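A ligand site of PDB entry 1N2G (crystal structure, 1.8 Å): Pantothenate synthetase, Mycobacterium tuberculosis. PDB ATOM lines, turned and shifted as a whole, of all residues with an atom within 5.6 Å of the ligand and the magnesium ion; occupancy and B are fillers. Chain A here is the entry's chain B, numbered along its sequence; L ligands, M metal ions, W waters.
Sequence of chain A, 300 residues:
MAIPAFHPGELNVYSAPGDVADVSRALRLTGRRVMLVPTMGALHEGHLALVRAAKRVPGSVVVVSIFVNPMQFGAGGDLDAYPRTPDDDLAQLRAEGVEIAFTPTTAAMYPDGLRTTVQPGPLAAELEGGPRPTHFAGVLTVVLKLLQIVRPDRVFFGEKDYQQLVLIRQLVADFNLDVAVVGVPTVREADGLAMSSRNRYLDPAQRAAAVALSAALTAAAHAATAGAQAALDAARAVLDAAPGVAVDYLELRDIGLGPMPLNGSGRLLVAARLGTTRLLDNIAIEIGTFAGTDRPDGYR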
ATOM      1  N   PRO A  38     -10.436 -13.238 -25.627  1.00  0.00           N
ATOM      2  CA  PRO A  38     -10.360 -12.738 -24.255  1.00  0.00           C
ATOM      3  C   PRO A  38     -11.750 -12.444 -23.679  1.00  0.00           C
ATOM      4  O   PRO A  38     -12.569 -11.781 -24.316  1.00  0.00           O
ATOM      5  CB  PRO A  38      -9.532 -11.451 -24.387  1.00  0.00           C
ATOM      6  CG  PRO A  38      -8.782 -11.629 -25.714  1.00  0.00           C
ATOM      7  CD  PRO A  38      -9.801 -12.297 -26.571  1.00  0.00           C
ATOM      8  N   THR A  39     -12.003 -12.937 -22.468  1.00  0.00           N
ATOM      9  CA  THR A  39     -13.298 -12.692 -21.804  1.00  0.00           C
ATOM     10  C   THR A  39     -13.113 -12.499 -20.302  1.00  0.00           C
ATOM     11  O   THR A  39     -12.022 -12.674 -19.758  1.00  0.00           O
ATOM     12  CB  THR A  39     -14.328 -13.867 -21.999  1.00  0.00           C
ATOM     13  OG1 THR A  39     -14.083 -14.916 -21.045  1.00  0.00           O
ATOM     14  CG2 THR A  39     -14.258 -14.446 -23.400  1.00  0.00           C
ATOM     15  N   MET A  40     -14.197 -12.120 -19.641  1.00  0.00           N
ATOM     16  CA  MET A  40     -14.204 -11.967 -18.201  1.00  0.00           C
ATOM     17  C   MET A  40     -15.234 -12.944 -17.620  1.00  0.00           C
ATOM     18  O   MET A  40     -15.782 -12.742 -16.536  1.00  0.00           O
ATOM     19  CB  MET A  40     -14.524 -10.533 -17.803  1.00  0.00           C
ATOM     20  CG  MET A  40     -13.570  -9.553 -18.458  1.00  0.00           C
ATOM     21  SD  MET A  40     -13.175  -8.139 -17.447  1.00  0.00           S
ATOM     22  CE  MET A  40     -14.710  -7.276 -17.512  1.00  0.00           C
ATOM     23  N   GLY A  41     -15.491 -14.007 -18.372  1.00  0.00           N
ATOM     24  CA  GLY A  41     -16.435 -15.017 -17.911  1.00  0.00           C
ATOM     25  C   GLY A  41     -17.894 -14.619 -18.004  1.00  0.00           C
ATOM     26  O   GLY A  41     -18.233 -13.629 -18.653  1.00  0.00           O
ATOM     27  N   HIS A  44     -22.136 -15.678 -22.545  1.00  0.00           N
ATOM     28  CA  HIS A  44     -23.457 -15.753 -23.162  1.00  0.00           C
ATOM     29  C   HIS A  44     -23.281 -15.875 -24.679  1.00  0.00           C
ATOM     30  O   HIS A  44     -22.156 -15.925 -25.170  1.00  0.00           O
ATOM     31  CB  HIS A  44     -24.315 -14.547 -22.800  1.00  0.00           C
ATOM     32  CG  HIS A  44     -23.696 -13.225 -23.139  1.00  0.00           C
ATOM     33  ND1 HIS A  44     -23.374 -12.865 -24.428  1.00  0.00           N
ATOM     34  CD2 HIS A  44     -23.364 -12.175 -22.360  1.00  0.00           C
ATOM     35  CE1 HIS A  44     -22.884 -11.637 -24.427  1.00  0.00           C
ATOM     36  NE2 HIS A  44     -22.860 -11.196 -23.184  1.00  0.00           N
ATOM     37  N   GLY A  46     -23.283 -13.923 -27.019  1.00  0.00           N
ATOM     38  CA  GLY A  46     -22.385 -12.966 -27.639  1.00  0.00           C
ATOM     39  C   GLY A  46     -20.959 -13.511 -27.611  1.00  0.00           C
ATOM     40  O   GLY A  46     -20.240 -13.469 -28.620  1.00  0.00           O
ATOM     41  N   HIS A  47     -20.532 -14.025 -26.458  1.00  0.00           N
ATOM     42  CA  HIS A  47     -19.179 -14.580 -26.355  1.00  0.00           C
ATOM     43  C   HIS A  47     -19.036 -15.780 -27.264  1.00  0.00           C
ATOM     44  O   HIS A  47     -17.966 -15.980 -27.844  1.00  0.00           O
ATOM     45  CB  HIS A  47     -18.832 -15.049 -24.950  1.00  0.00           C
ATOM     46  CG  HIS A  47     -18.947 -13.986 -23.902  1.00  0.00           C
ATOM     47  ND1 HIS A  47     -20.114 -13.770 -23.210  1.00  0.00           N
ATOM     48  CD2 HIS A  47     -18.059 -13.083 -23.440  1.00  0.00           C
ATOM     49  CE1 HIS A  47     -19.939 -12.771 -22.364  1.00  0.00           C
ATOM     50  NE2 HIS A  47     -18.693 -12.331 -22.478  1.00  0.00           N
ATOM     51  N   ALA A  49     -20.320 -16.318 -30.113  1.00  0.00           N
ATOM     52  CA  ALA A  49     -20.135 -15.924 -31.502  1.00  0.00           C
ATOM     53  C   ALA A  49     -18.642 -15.713 -31.754  1.00  0.00           C
ATOM     54  O   ALA A  49     -18.144 -16.054 -32.843  1.00  0.00           O
ATOM     55  CB  ALA A  49     -20.913 -14.649 -31.806  1.00  0.00           C
ATOM     56  N   LEU A  50     -17.933 -15.147 -30.769  1.00  0.00           N
ATOM     57  CA  LEU A  50     -16.482 -14.959 -30.900  1.00  0.00           C
ATOM     58  C   LEU A  50     -15.805 -16.328 -30.961  1.00  0.00           C
ATOM     59  O   LEU A  50     -14.932 -16.565 -31.800  1.00  0.00           O
ATOM     60  CB  LEU A  50     -15.921 -14.159 -29.700  1.00  0.00           C
ATOM     61  CG  LEU A  50     -15.909 -12.626 -29.842  1.00  0.00           C
ATOM     62  CD1 LEU A  50     -17.256 -12.125 -30.213  1.00  0.00           C
ATOM     63  CD2 LEU A  50     -15.457 -11.983 -28.533  1.00  0.00           C
ATOM     64  N   TYR A  82     -18.787  -8.209  -9.713  1.00  0.00           N
ATOM     65  CA  TYR A  82     -18.791  -8.855 -11.015  1.00  0.00           C
ATOM     66  C   TYR A  82     -19.200 -10.321 -10.911  1.00  0.00           C
ATOM     67  O   TYR A  82     -18.671 -11.070 -10.087  1.00  0.00           O
ATOM     68  CB  TYR A  82     -17.418  -8.759 -11.671  1.00  0.00           C
ATOM     69  CG  TYR A  82     -17.482  -8.851 -13.172  1.00  0.00           C
ATOM     70  CD1 TYR A  82     -17.929  -7.764 -13.929  1.00  0.00           C
ATOM     71  CD2 TYR A  82     -17.143 -10.029 -13.848  1.00  0.00           C
ATOM     72  CE1 TYR A  82     -18.036  -7.847 -15.314  1.00  0.00           C
ATOM     73  CE2 TYR A  82     -17.256 -10.123 -15.227  1.00  0.00           C
ATOM     74  CZ  TYR A  82     -17.703  -9.032 -15.960  1.00  0.00           C
ATOM     75  OH  TYR A  82     -17.828  -9.115 -17.332  1.00  0.00           O
ATOM     76  N   PHE A 156      -9.843 -12.231 -31.097  1.00  0.00           N
ATOM     77  CA  PHE A 156     -11.223 -11.850 -31.380  1.00  0.00           C
ATOM     78  C   PHE A 156     -11.898 -10.965 -30.349  1.00  0.00           C
ATOM     79  O   PHE A 156     -11.843 -11.239 -29.144  1.00  0.00           O
ATOM     80  CB  PHE A 156     -12.073 -13.126 -31.567  1.00  0.00           C
ATOM     81  CG  PHE A 156     -11.578 -14.018 -32.672  1.00  0.00           C
ATOM     82  CD1 PHE A 156     -10.378 -14.722 -32.527  1.00  0.00           C
ATOM     83  CD2 PHE A 156     -12.250 -14.087 -33.872  1.00  0.00           C
ATOM     84  CE1 PHE A 156      -9.853 -15.482 -33.593  1.00  0.00           C
ATOM     85  CE2 PHE A 156     -11.741 -14.834 -34.944  1.00  0.00           C
ATOM     86  CZ  PHE A 156     -10.535 -15.526 -34.806  1.00  0.00           C
ATOM     87  N   PHE A 157     -12.554  -9.909 -30.832  1.00  0.00           N
ATOM     88  CA  PHE A 157     -13.283  -8.971 -29.969  1.00  0.00           C
ATOM     89  C   PHE A 157     -14.605  -8.632 -30.641  1.00  0.00           C
ATOM     90  O   PHE A 157     -14.706  -8.609 -31.856  1.00  0.00           O
ATOM     91  CB  PHE A 157     -12.484  -7.670 -29.782  1.00  0.00           C
ATOM     92  CG  PHE A 157     -11.205  -7.858 -29.027  1.00  0.00           C
ATOM     93  CD1 PHE A 157     -10.018  -8.053 -29.682  1.00  0.00           C
ATOM     94  CD2 PHE A 157     -11.213  -7.851 -27.624  1.00  0.00           C
ATOM     95  CE1 PHE A 157      -8.808  -8.255 -28.977  1.00  0.00           C
ATOM     96  CE2 PHE A 157     -10.021  -8.054 -26.906  1.00  0.00           C
ATOM     97  CZ  PHE A 157      -8.820  -8.244 -27.587  1.00  0.00           C
ATOM     98  N   GLY A 158     -15.630  -8.342 -29.839  1.00  0.00           N
ATOM     99  CA  GLY A 158     -16.913  -8.056 -30.430  1.00  0.00           C
ATOM    100  C   GLY A 158     -17.041  -6.611 -30.855  1.00  0.00           C
ATOM    101  O   GLY A 158     -16.477  -5.716 -30.221  1.00  0.00           O
ATOM    102  N   GLU A 159     -17.773  -6.380 -31.943  1.00  0.00           N
ATOM    103  CA  GLU A 159     -17.972  -5.010 -32.418  1.00  0.00           C
ATOM    104  C   GLU A 159     -18.813  -4.203 -31.475  1.00  0.00           C
ATOM    105  O   GLU A 159     -18.831  -2.980 -31.549  1.00  0.00           O
ATOM    106  CB  GLU A 159     -18.646  -5.000 -33.788  1.00  0.00           C
ATOM    107  CG  GLU A 159     -17.684  -5.476 -34.884  1.00  0.00           C
ATOM    108  CD  GLU A 159     -18.278  -5.337 -36.270  1.00  0.00           C
ATOM    109  OE1 GLU A 159     -19.465  -5.010 -36.393  1.00  0.00           O
ATOM    110  OE2 GLU A 159     -17.541  -5.580 -37.250  1.00  0.00           O
ATOM    111  N   LYS A 160     -19.539  -4.878 -30.579  1.00  0.00           N
ATOM    112  CA  LYS A 160     -20.377  -4.145 -29.626  1.00  0.00           C
ATOM    113  C   LYS A 160     -19.533  -3.102 -28.899  1.00  0.00           C
ATOM    114  O   LYS A 160     -19.982  -1.978 -28.668  1.00  0.00           O
ATOM    115  CB  LYS A 160     -20.990  -5.098 -28.592  1.00  0.00           C
ATOM    116  CG  LYS A 160     -22.124  -4.443 -27.807  1.00  0.00           C
ATOM    117  CD  LYS A 160     -22.541  -5.286 -26.617  1.00  0.00           C
ATOM    118  CE  LYS A 160     -21.402  -5.440 -25.633  1.00  0.00           C
ATOM    119  NZ  LYS A 160     -21.861  -6.197 -24.439  1.00  0.00           N
ATOM    120  N   ASP A 161     -18.318  -3.471 -28.506  1.00  0.00           N
ATOM    121  CA  ASP A 161     -17.449  -2.490 -27.835  1.00  0.00           C
ATOM    122  C   ASP A 161     -16.520  -1.979 -28.915  1.00  0.00           C
ATOM    123  O   ASP A 161     -15.316  -2.268 -28.925  1.00  0.00           O
ATOM    124  CB  ASP A 161     -16.702  -3.172 -26.713  1.00  0.00           C
ATOM    125  CG  ASP A 161     -17.645  -3.725 -25.669  1.00  0.00           C
ATOM    126  OD1 ASP A 161     -18.216  -2.919 -24.929  1.00  0.00           O
ATOM    127  OD2 ASP A 161     -17.843  -4.957 -25.643  1.00  0.00           O
ATOM    128  N   GLN A 164     -13.331  -0.056 -27.934  1.00  0.00           N
ATOM    129  CA  GLN A 164     -12.352  -1.015 -27.424  1.00  0.00           C
ATOM    130  C   GLN A 164     -11.634  -1.684 -28.613  1.00  0.00           C
ATOM    131  O   GLN A 164     -10.410  -1.754 -28.644  1.00  0.00           O
ATOM    132  CB  GLN A 164     -13.050  -2.100 -26.595  1.00  0.00           C
ATOM    133  CG  GLN A 164     -12.154  -3.312 -26.344  1.00  0.00           C
ATOM    134  CD  GLN A 164     -12.755  -4.238 -25.299  1.00  0.00           C
ATOM    135  OE1 GLN A 164     -12.687  -3.942 -24.115  1.00  0.00           O
ATOM    136  NE2 GLN A 164     -13.347  -5.340 -25.732  1.00  0.00           N
ATOM    137  N   VAL A 184     -15.892  -9.120 -34.408  1.00  0.00           N
ATOM    138  CA  VAL A 184     -17.020 -10.007 -34.651  1.00  0.00           C
ATOM    139  C   VAL A 184     -18.334  -9.232 -34.466  1.00  0.00           C
ATOM    140  O   VAL A 184     -18.489  -8.502 -33.474  1.00  0.00           O
ATOM    141  CB  VAL A 184     -16.990 -11.187 -33.661  1.00  0.00           C
ATOM    142  CG1 VAL A 184     -18.210 -12.094 -33.865  1.00  0.00           C
ATOM    143  CG2 VAL A 184     -15.684 -11.946 -33.824  1.00  0.00           C
ATOM    144  N   PRO A 185     -19.257  -9.360 -35.431  1.00  0.00           N
ATOM    145  CA  PRO A 185     -20.556  -8.665 -35.401  1.00  0.00           C
ATOM    146  C   PRO A 185     -21.322  -8.883 -34.093  1.00  0.00           C
ATOM    147  O   PRO A 185     -21.322  -9.979 -33.515  1.00  0.00           O
ATOM    148  CB  PRO A 185     -21.300  -9.252 -36.602  1.00  0.00           C
ATOM    149  CG  PRO A 185     -20.179  -9.526 -37.568  1.00  0.00           C
ATOM    150  CD  PRO A 185     -19.107 -10.135 -36.686  1.00  0.00           C
ATOM    151  N   THR A 186     -21.979  -7.827 -33.651  1.00  0.00           N
ATOM    152  CA  THR A 186     -22.735  -7.886 -32.413  1.00  0.00           C
ATOM    153  C   THR A 186     -23.918  -8.838 -32.479  1.00  0.00           C
ATOM    154  O   THR A 186     -24.705  -8.809 -33.426  1.00  0.00           O
ATOM    155  CB  THR A 186     -23.236  -6.469 -32.045  1.00  0.00           C
ATOM    156  OG1 THR A 186     -22.082  -5.640 -31.832  1.00  0.00           O
ATOM    157  CG2 THR A 186     -24.072  -6.479 -30.760  1.00  0.00           C
ATOM    158  N   VAL A 187     -24.015  -9.702 -31.467  1.00  0.00           N
ATOM    159  CA  VAL A 187     -25.111 -10.649 -31.361  1.00  0.00           C
ATOM    160  C   VAL A 187     -26.212  -9.880 -30.643  1.00  0.00           C
ATOM    161  O   VAL A 187     -25.958  -9.190 -29.647  1.00  0.00           O
ATOM    162  CB  VAL A 187     -24.682 -11.883 -30.536  1.00  0.00           C
ATOM    163  CG1 VAL A 187     -25.866 -12.807 -30.312  1.00  0.00           C
ATOM    164  CG2 VAL A 187     -23.579 -12.628 -31.273  1.00  0.00           C
ATOM    165  N   ARG A 188     -27.433  -9.988 -31.155  1.00  0.00           N
ATOM    166  CA  ARG A 188     -28.560  -9.251 -30.604  1.00  0.00           C
ATOM    167  C   ARG A 188     -29.755 -10.112 -30.238  1.00  0.00           C
ATOM    168  O   ARG A 188     -29.971 -11.181 -30.799  1.00  0.00           O
ATOM    169  CB  ARG A 188     -29.032  -8.224 -31.636  1.00  0.00           C
ATOM    170  CG  ARG A 188     -27.953  -7.264 -32.069  1.00  0.00           C
ATOM    171  CD  ARG A 188     -28.375  -6.367 -33.234  1.00  0.00           C
ATOM    172  NE  ARG A 188     -27.310  -5.412 -33.549  1.00  0.00           N
ATOM    173  CZ  ARG A 188     -27.050  -4.320 -32.836  1.00  0.00           C
ATOM    174  NH1 ARG A 188     -27.789  -4.011 -31.777  1.00  0.00           N
ATOM    175  NH2 ARG A 188     -26.000  -3.567 -33.160  1.00  0.00           N
ATOM    176  N   ALA A 194     -28.556  -5.264 -28.133  1.00  0.00           N
ATOM    177  CA  ALA A 194     -27.247  -5.908 -28.115  1.00  0.00           C
ATOM    178  C   ALA A 194     -27.148  -6.793 -26.866  1.00  0.00           C
ATOM    179  O   ALA A 194     -27.408  -6.318 -25.744  1.00  0.00           O
ATOM    180  CB  ALA A 194     -26.160  -4.870 -28.073  1.00  0.00           C
ATOM    181  N   MET A 195     -26.790  -8.078 -27.025  1.00  0.00           N
ATOM    182  CA  MET A 195     -26.697  -8.937 -25.843  1.00  0.00           C
ATOM    183  C   MET A 195     -25.593  -8.467 -24.919  1.00  0.00           C
ATOM    184  O   MET A 195     -24.506  -8.074 -25.353  1.00  0.00           O
ATOM    185  CB  MET A 195     -26.451 -10.386 -26.237  1.00  0.00           C
ATOM    186  CG  MET A 195     -27.684 -11.095 -26.768  1.00  0.00           C
ATOM    187  SD  MET A 195     -27.368 -12.855 -26.996  1.00  0.00           S
ATOM    188  CE  MET A 195     -28.657 -13.235 -28.152  1.00  0.00           C
ATOM    189  N   SER A 196     -25.887  -8.493 -23.615  1.00  0.00           N
ATOM    190  CA  SER A 196     -24.934  -8.054 -22.626  1.00  0.00           C
ATOM    191  C   SER A 196     -25.409  -8.651 -21.310  1.00  0.00           C
ATOM    192  O   SER A 196     -26.623  -8.771 -21.078  1.00  0.00           O
ATOM    193  CB  SER A 196     -24.927  -6.527 -22.554  1.00  0.00           C
ATOM    194  OG  SER A 196     -23.678  -6.029 -22.097  1.00  0.00           O
ATOM    195  N   SER A 197     -24.466  -9.025 -20.455  1.00  0.00           N
ATOM    196  CA  SER A 197     -24.815  -9.619 -19.163  1.00  0.00           C
ATOM    197  C   SER A 197     -25.614  -8.614 -18.337  1.00  0.00           C
ATOM    198  O   SER A 197     -26.505  -8.986 -17.578  1.00  0.00           O
ATOM    199  CB  SER A 197     -23.539 -10.024 -18.402  1.00  0.00           C
ATOM    200  OG  SER A 197     -22.715 -10.870 -19.211  1.00  0.00           O
ATOM    201  N   ARG A 198     -25.308  -7.333 -18.493  1.00  0.00           N
ATOM    202  CA  ARG A 198     -26.011  -6.302 -17.736  1.00  0.00           C
ATOM    203  C   ARG A 198     -27.478  -6.076 -18.115  1.00  0.00           C
ATOM    204  O   ARG A 198     -28.210  -5.393 -17.400  1.00  0.00           O
ATOM    205  CB  ARG A 198     -25.225  -4.981 -17.815  1.00  0.00           C
ATOM    206  CG  ARG A 198     -25.218  -4.339 -19.176  1.00  0.00           C
ATOM    207  CD  ARG A 198     -24.379  -3.081 -19.181  1.00  0.00           C
ATOM    208  NE  ARG A 198     -22.951  -3.372 -19.280  1.00  0.00           N
ATOM    209  CZ  ARG A 198     -21.999  -2.481 -19.071  1.00  0.00           C
ATOM    210  NH1 ARG A 198     -22.300  -1.229 -18.740  1.00  0.00           N
ATOM    211  NH2 ARG A 198     -20.721  -2.830 -19.213  1.00  0.00           N
ATOM    212  N   ASN A 199     -27.949  -6.682 -19.210  1.00  0.00           N
ATOM    213  CA  ASN A 199     -29.336  -6.520 -19.615  1.00  0.00           C
ATOM    214  C   ASN A 199     -30.317  -7.085 -18.594  1.00  0.00           C
ATOM    215  O   ASN A 199     -31.460  -6.645 -18.503  1.00  0.00           O
ATOM    216  CB  ASN A 199     -29.637  -7.221 -20.957  1.00  0.00           C
ATOM    217  CG  ASN A 199     -28.983  -6.532 -22.163  1.00  0.00           C
ATOM    218  OD1 ASN A 199     -28.556  -5.399 -22.075  1.00  0.00           O
ATOM    219  ND2 ASN A 199     -28.934  -7.240 -23.299  1.00  0.00           N
HETATM  220  P1  LIG L   1     -20.885  -6.465 -19.547  1.00  0.00           P
HETATM  221  O1  LIG L   1     -20.163  -5.278 -20.244  1.00  0.00           O
HETATM  222  O2  LIG L   1     -20.457  -6.555 -18.034  1.00  0.00           O
HETATM  223  O3  LIG L   1     -22.438  -6.309 -19.664  1.00  0.00           O
HETATM  224  P2  LIG L   1     -20.112  -8.259 -21.758  1.00  0.00           P
HETATM  225  O4  LIG L   1     -21.427  -8.929 -22.246  1.00  0.00           O
HETATM  226  O5  LIG L   1     -19.781  -7.111 -22.713  1.00  0.00           O
HETATM  227  O6  LIG L   1     -20.382  -7.801 -20.233  1.00  0.00           O
HETATM  228  P3  LIG L   1     -17.516  -8.609 -21.493  1.00  0.00           P
HETATM  229  O7  LIG L   1     -16.690  -9.398 -20.622  1.00  0.00           O
HETATM  230  O8  LIG L   1     -17.644  -7.235 -21.049  1.00  0.00           O
HETATM  231  C1  LIG L   1     -18.935  -9.248 -21.709  1.00  0.00           C
HETATM  232  O9  LIG L   1     -16.632  -8.649 -22.943  1.00  0.00           O
HETATM  233  C2  LIG L   1     -16.049  -9.861 -23.485  1.00  0.00           C
HETATM  234  C3  LIG L   1     -15.962  -9.932 -25.052  1.00  0.00           C
HETATM  235  O10 LIG L   1     -17.255 -10.364 -25.600  1.00  0.00           O
HETATM  236  C4  LIG L   1     -15.676  -8.558 -25.751  1.00  0.00           C
HETATM  237  O11 LIG L   1     -14.829  -8.766 -26.941  1.00  0.00           O
HETATM  238  C5  LIG L   1     -17.030  -8.084 -26.095  1.00  0.00           C
HETATM  239  O12 LIG L   1     -17.022  -7.027 -27.053  1.00  0.00           O
HETATM  240  C6  LIG L   1     -17.690  -9.387 -26.565  1.00  0.00           C
HETATM  241  N1  LIG L   1     -19.150  -9.244 -26.577  1.00  0.00           N
HETATM  242  C7  LIG L   1     -20.000  -8.915 -25.561  1.00  0.00           C
HETATM  243  N2  LIG L   1     -21.265  -8.830 -25.858  1.00  0.00           N
HETATM  244  C8  LIG L   1     -21.263  -9.135 -27.213  1.00  0.00           C
HETATM  245  C9  LIG L   1     -22.298  -9.211 -28.182  1.00  0.00           C
HETATM  246  N3  LIG L   1     -23.578  -8.980 -27.878  1.00  0.00           N
HETATM  247  N4  LIG L   1     -21.949  -9.548 -29.496  1.00  0.00           N
HETATM  248  C10 LIG L   1     -20.625  -9.788 -29.824  1.00  0.00           C
HETATM  249  N5  LIG L   1     -19.573  -9.721 -28.962  1.00  0.00           N
HETATM  250  C11 LIG L   1     -19.959  -9.386 -27.667  1.00  0.00           C
HETATM  251 MG    MG M   1     -19.049  -5.535 -22.159  1.00  0.00          MG
HETATM  252  O   HOH W   1     -16.731 -11.801 -20.485  1.00  0.00           O
HETATM  253  O   HOH W   2     -20.230 -11.238 -19.144  1.00  0.00           O
HETATM  254  O   HOH W   3     -12.877 -10.442 -26.682  1.00  0.00           O
HETATM  255  O   HOH W   4     -19.564  -3.845 -22.917  1.00  0.00           O
HETATM  256  O   HOH W   5     -17.237  -5.530 -23.102  1.00  0.00           O
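A nitrogen (N3) of the ligand is in hydrogen-bond range of the backbone carbonyl oxygen (O) of Val 187 (3.0 Å). The side-chain amino group of Lys 160 lies within salt-bridge range of an oxygen (O4) of the ligand, 3.5 Å away. The backbone NH of Arg 198 lies within hydrogen-bond range of an oxygen (O3) of the ligand (3.3 Å). N of Val 187 sits at hydrogen-bond distance from N4 of the ligand, 2.9 Å away. O3 of the ligand is in salt-bridge range of NE of Arg 198 (3.0 Å). OD2 of Asp 161 sits at hydrogen-bond distance from O12 of the ligand (2.6 Å). O4 of the ligand sits at hydrogen-bond distance from NE2 of His 44 (2.8 Å). The backbone carbonyl oxygen of Met 195 is in hydrogen-bond range of a nitrogen (N3) of the ligand, at 2.8 Å. The side-chain hydroxyl (OH) of Tyr 82 sits at hydrogen-bond distance from an oxygen (O7) of the ligand, at 3.5 Å. The side-chain hydroxyl (OG) of Ser 196 sits at hydrogen-bond distance from an oxygen (O3) of the ligand, at 2.7 Å. The backbone carbonyl oxygen (O) of Gly 158 sits at hydrogen-bond distance from an oxygen (O12) of the ligand (3.5 Å). O3 of the ligand lies within hydrogen-bond range of N of Ser 197. An oxygen (O11) of the ligand lies within hydrogen-bond range of the backbone NH (N) of Gly 158 (3.0 Å).
The side-chain hydroxyl (OG) of Ser 196 sits at hydrogen-bond distance from the side-chain amino group (NZ) of Lys 160 (3.0 Å). The side-chain amino group of Lys 160 lies within hydrogen-bond range of the backbone carbonyl oxygen of Met 195 (3.4 Å). A ring nitrogen (ND1) of His 44 lies within hydrogen-bond range of the backbone NH (N) of Gly 46. N of Ser 196 lies close to ND2 of Asn 199, at 3.3 Å. The backbone NH of His 44 is in hydrogen-bond range of a ring nitrogen (ND1) of His 47 (2.9 Å). The backbone NH (N) of Lys 160 lies within hydrogen-bond range of the side-chain hydroxyl (OG1) of Thr 186 (2.9 Å). O of Val 187 sits at hydrogen-bond distance from N of Met 195 (3.0 Å). The backbone NH of Val 184 is in hydrogen-bond range of the backbone carbonyl oxygen of Phe 157.
Residues that only touch the ligand: Pro 38 (3.9 Å), Met 40 (3.7 Å), Gly 46 (3.8 Å), His 47 (3.2 Å), Leu 50 (3.6 Å), Phe 157 (3.4 Å), Gln 164 (3.9 Å), Pro 185 (3.8 Å) and Thr 186 (3.4 Å). Hydrophobic or aromatic side chains within 4 Å of the ligand: Met 40, His 44, His 47, Leu 50, Tyr 82, Phe 157, Val 187 and Met 195. Of the 28 residues printed, 19 come within 4 Å of the ligand.
Lys 160 touches the magnesium ion (NZ to MG, 3.7 Å). OD2 of Asp 161 touches the magnesium ion, at 3.7 Å. Of the 28 residues printed, 2 come within 4 Å of the magnesium ion. The nearest printed residue that does not touch the magnesium ion is Arg 198 (4.3 Å).
An oxygen (O5) of the ligand binds the magnesium ion (1.8 Å). Water W4 binds the magnesium ion, at 1.9 Å. Water W5 binds the magnesium ion (2.0 Å). O1 of the ligand is bound to the magnesium ion (2.2 Å). O8 of the ligand is bound to the magnesium ion (2.5 Å). The magnesium ion has five donor atoms within binding distance.
Water W5 lies within hydrogen-bond range of OD2 of Asp 161 and O9 of the ligand. Water W1 lies within hydrogen-bond range of an oxygen (O7) of the ligand (2.4 Å), the backbone NH of Met 40 (2.7 Å), a ring nitrogen (NE2) of His 47 (2.8 Å) and the backbone carbonyl oxygen of Gly 41 (3.0 Å). Water W3 lies within hydrogen-bond range of O11 of the ligand (2.6 Å), O of Pro 38 (2.7 Å) and O of Phe 156 (2.8 Å). Water W2 lies within hydrogen-bond range of the side-chain hydroxyl of Ser 197 and the backbone carbonyl oxygen of Gly 41.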
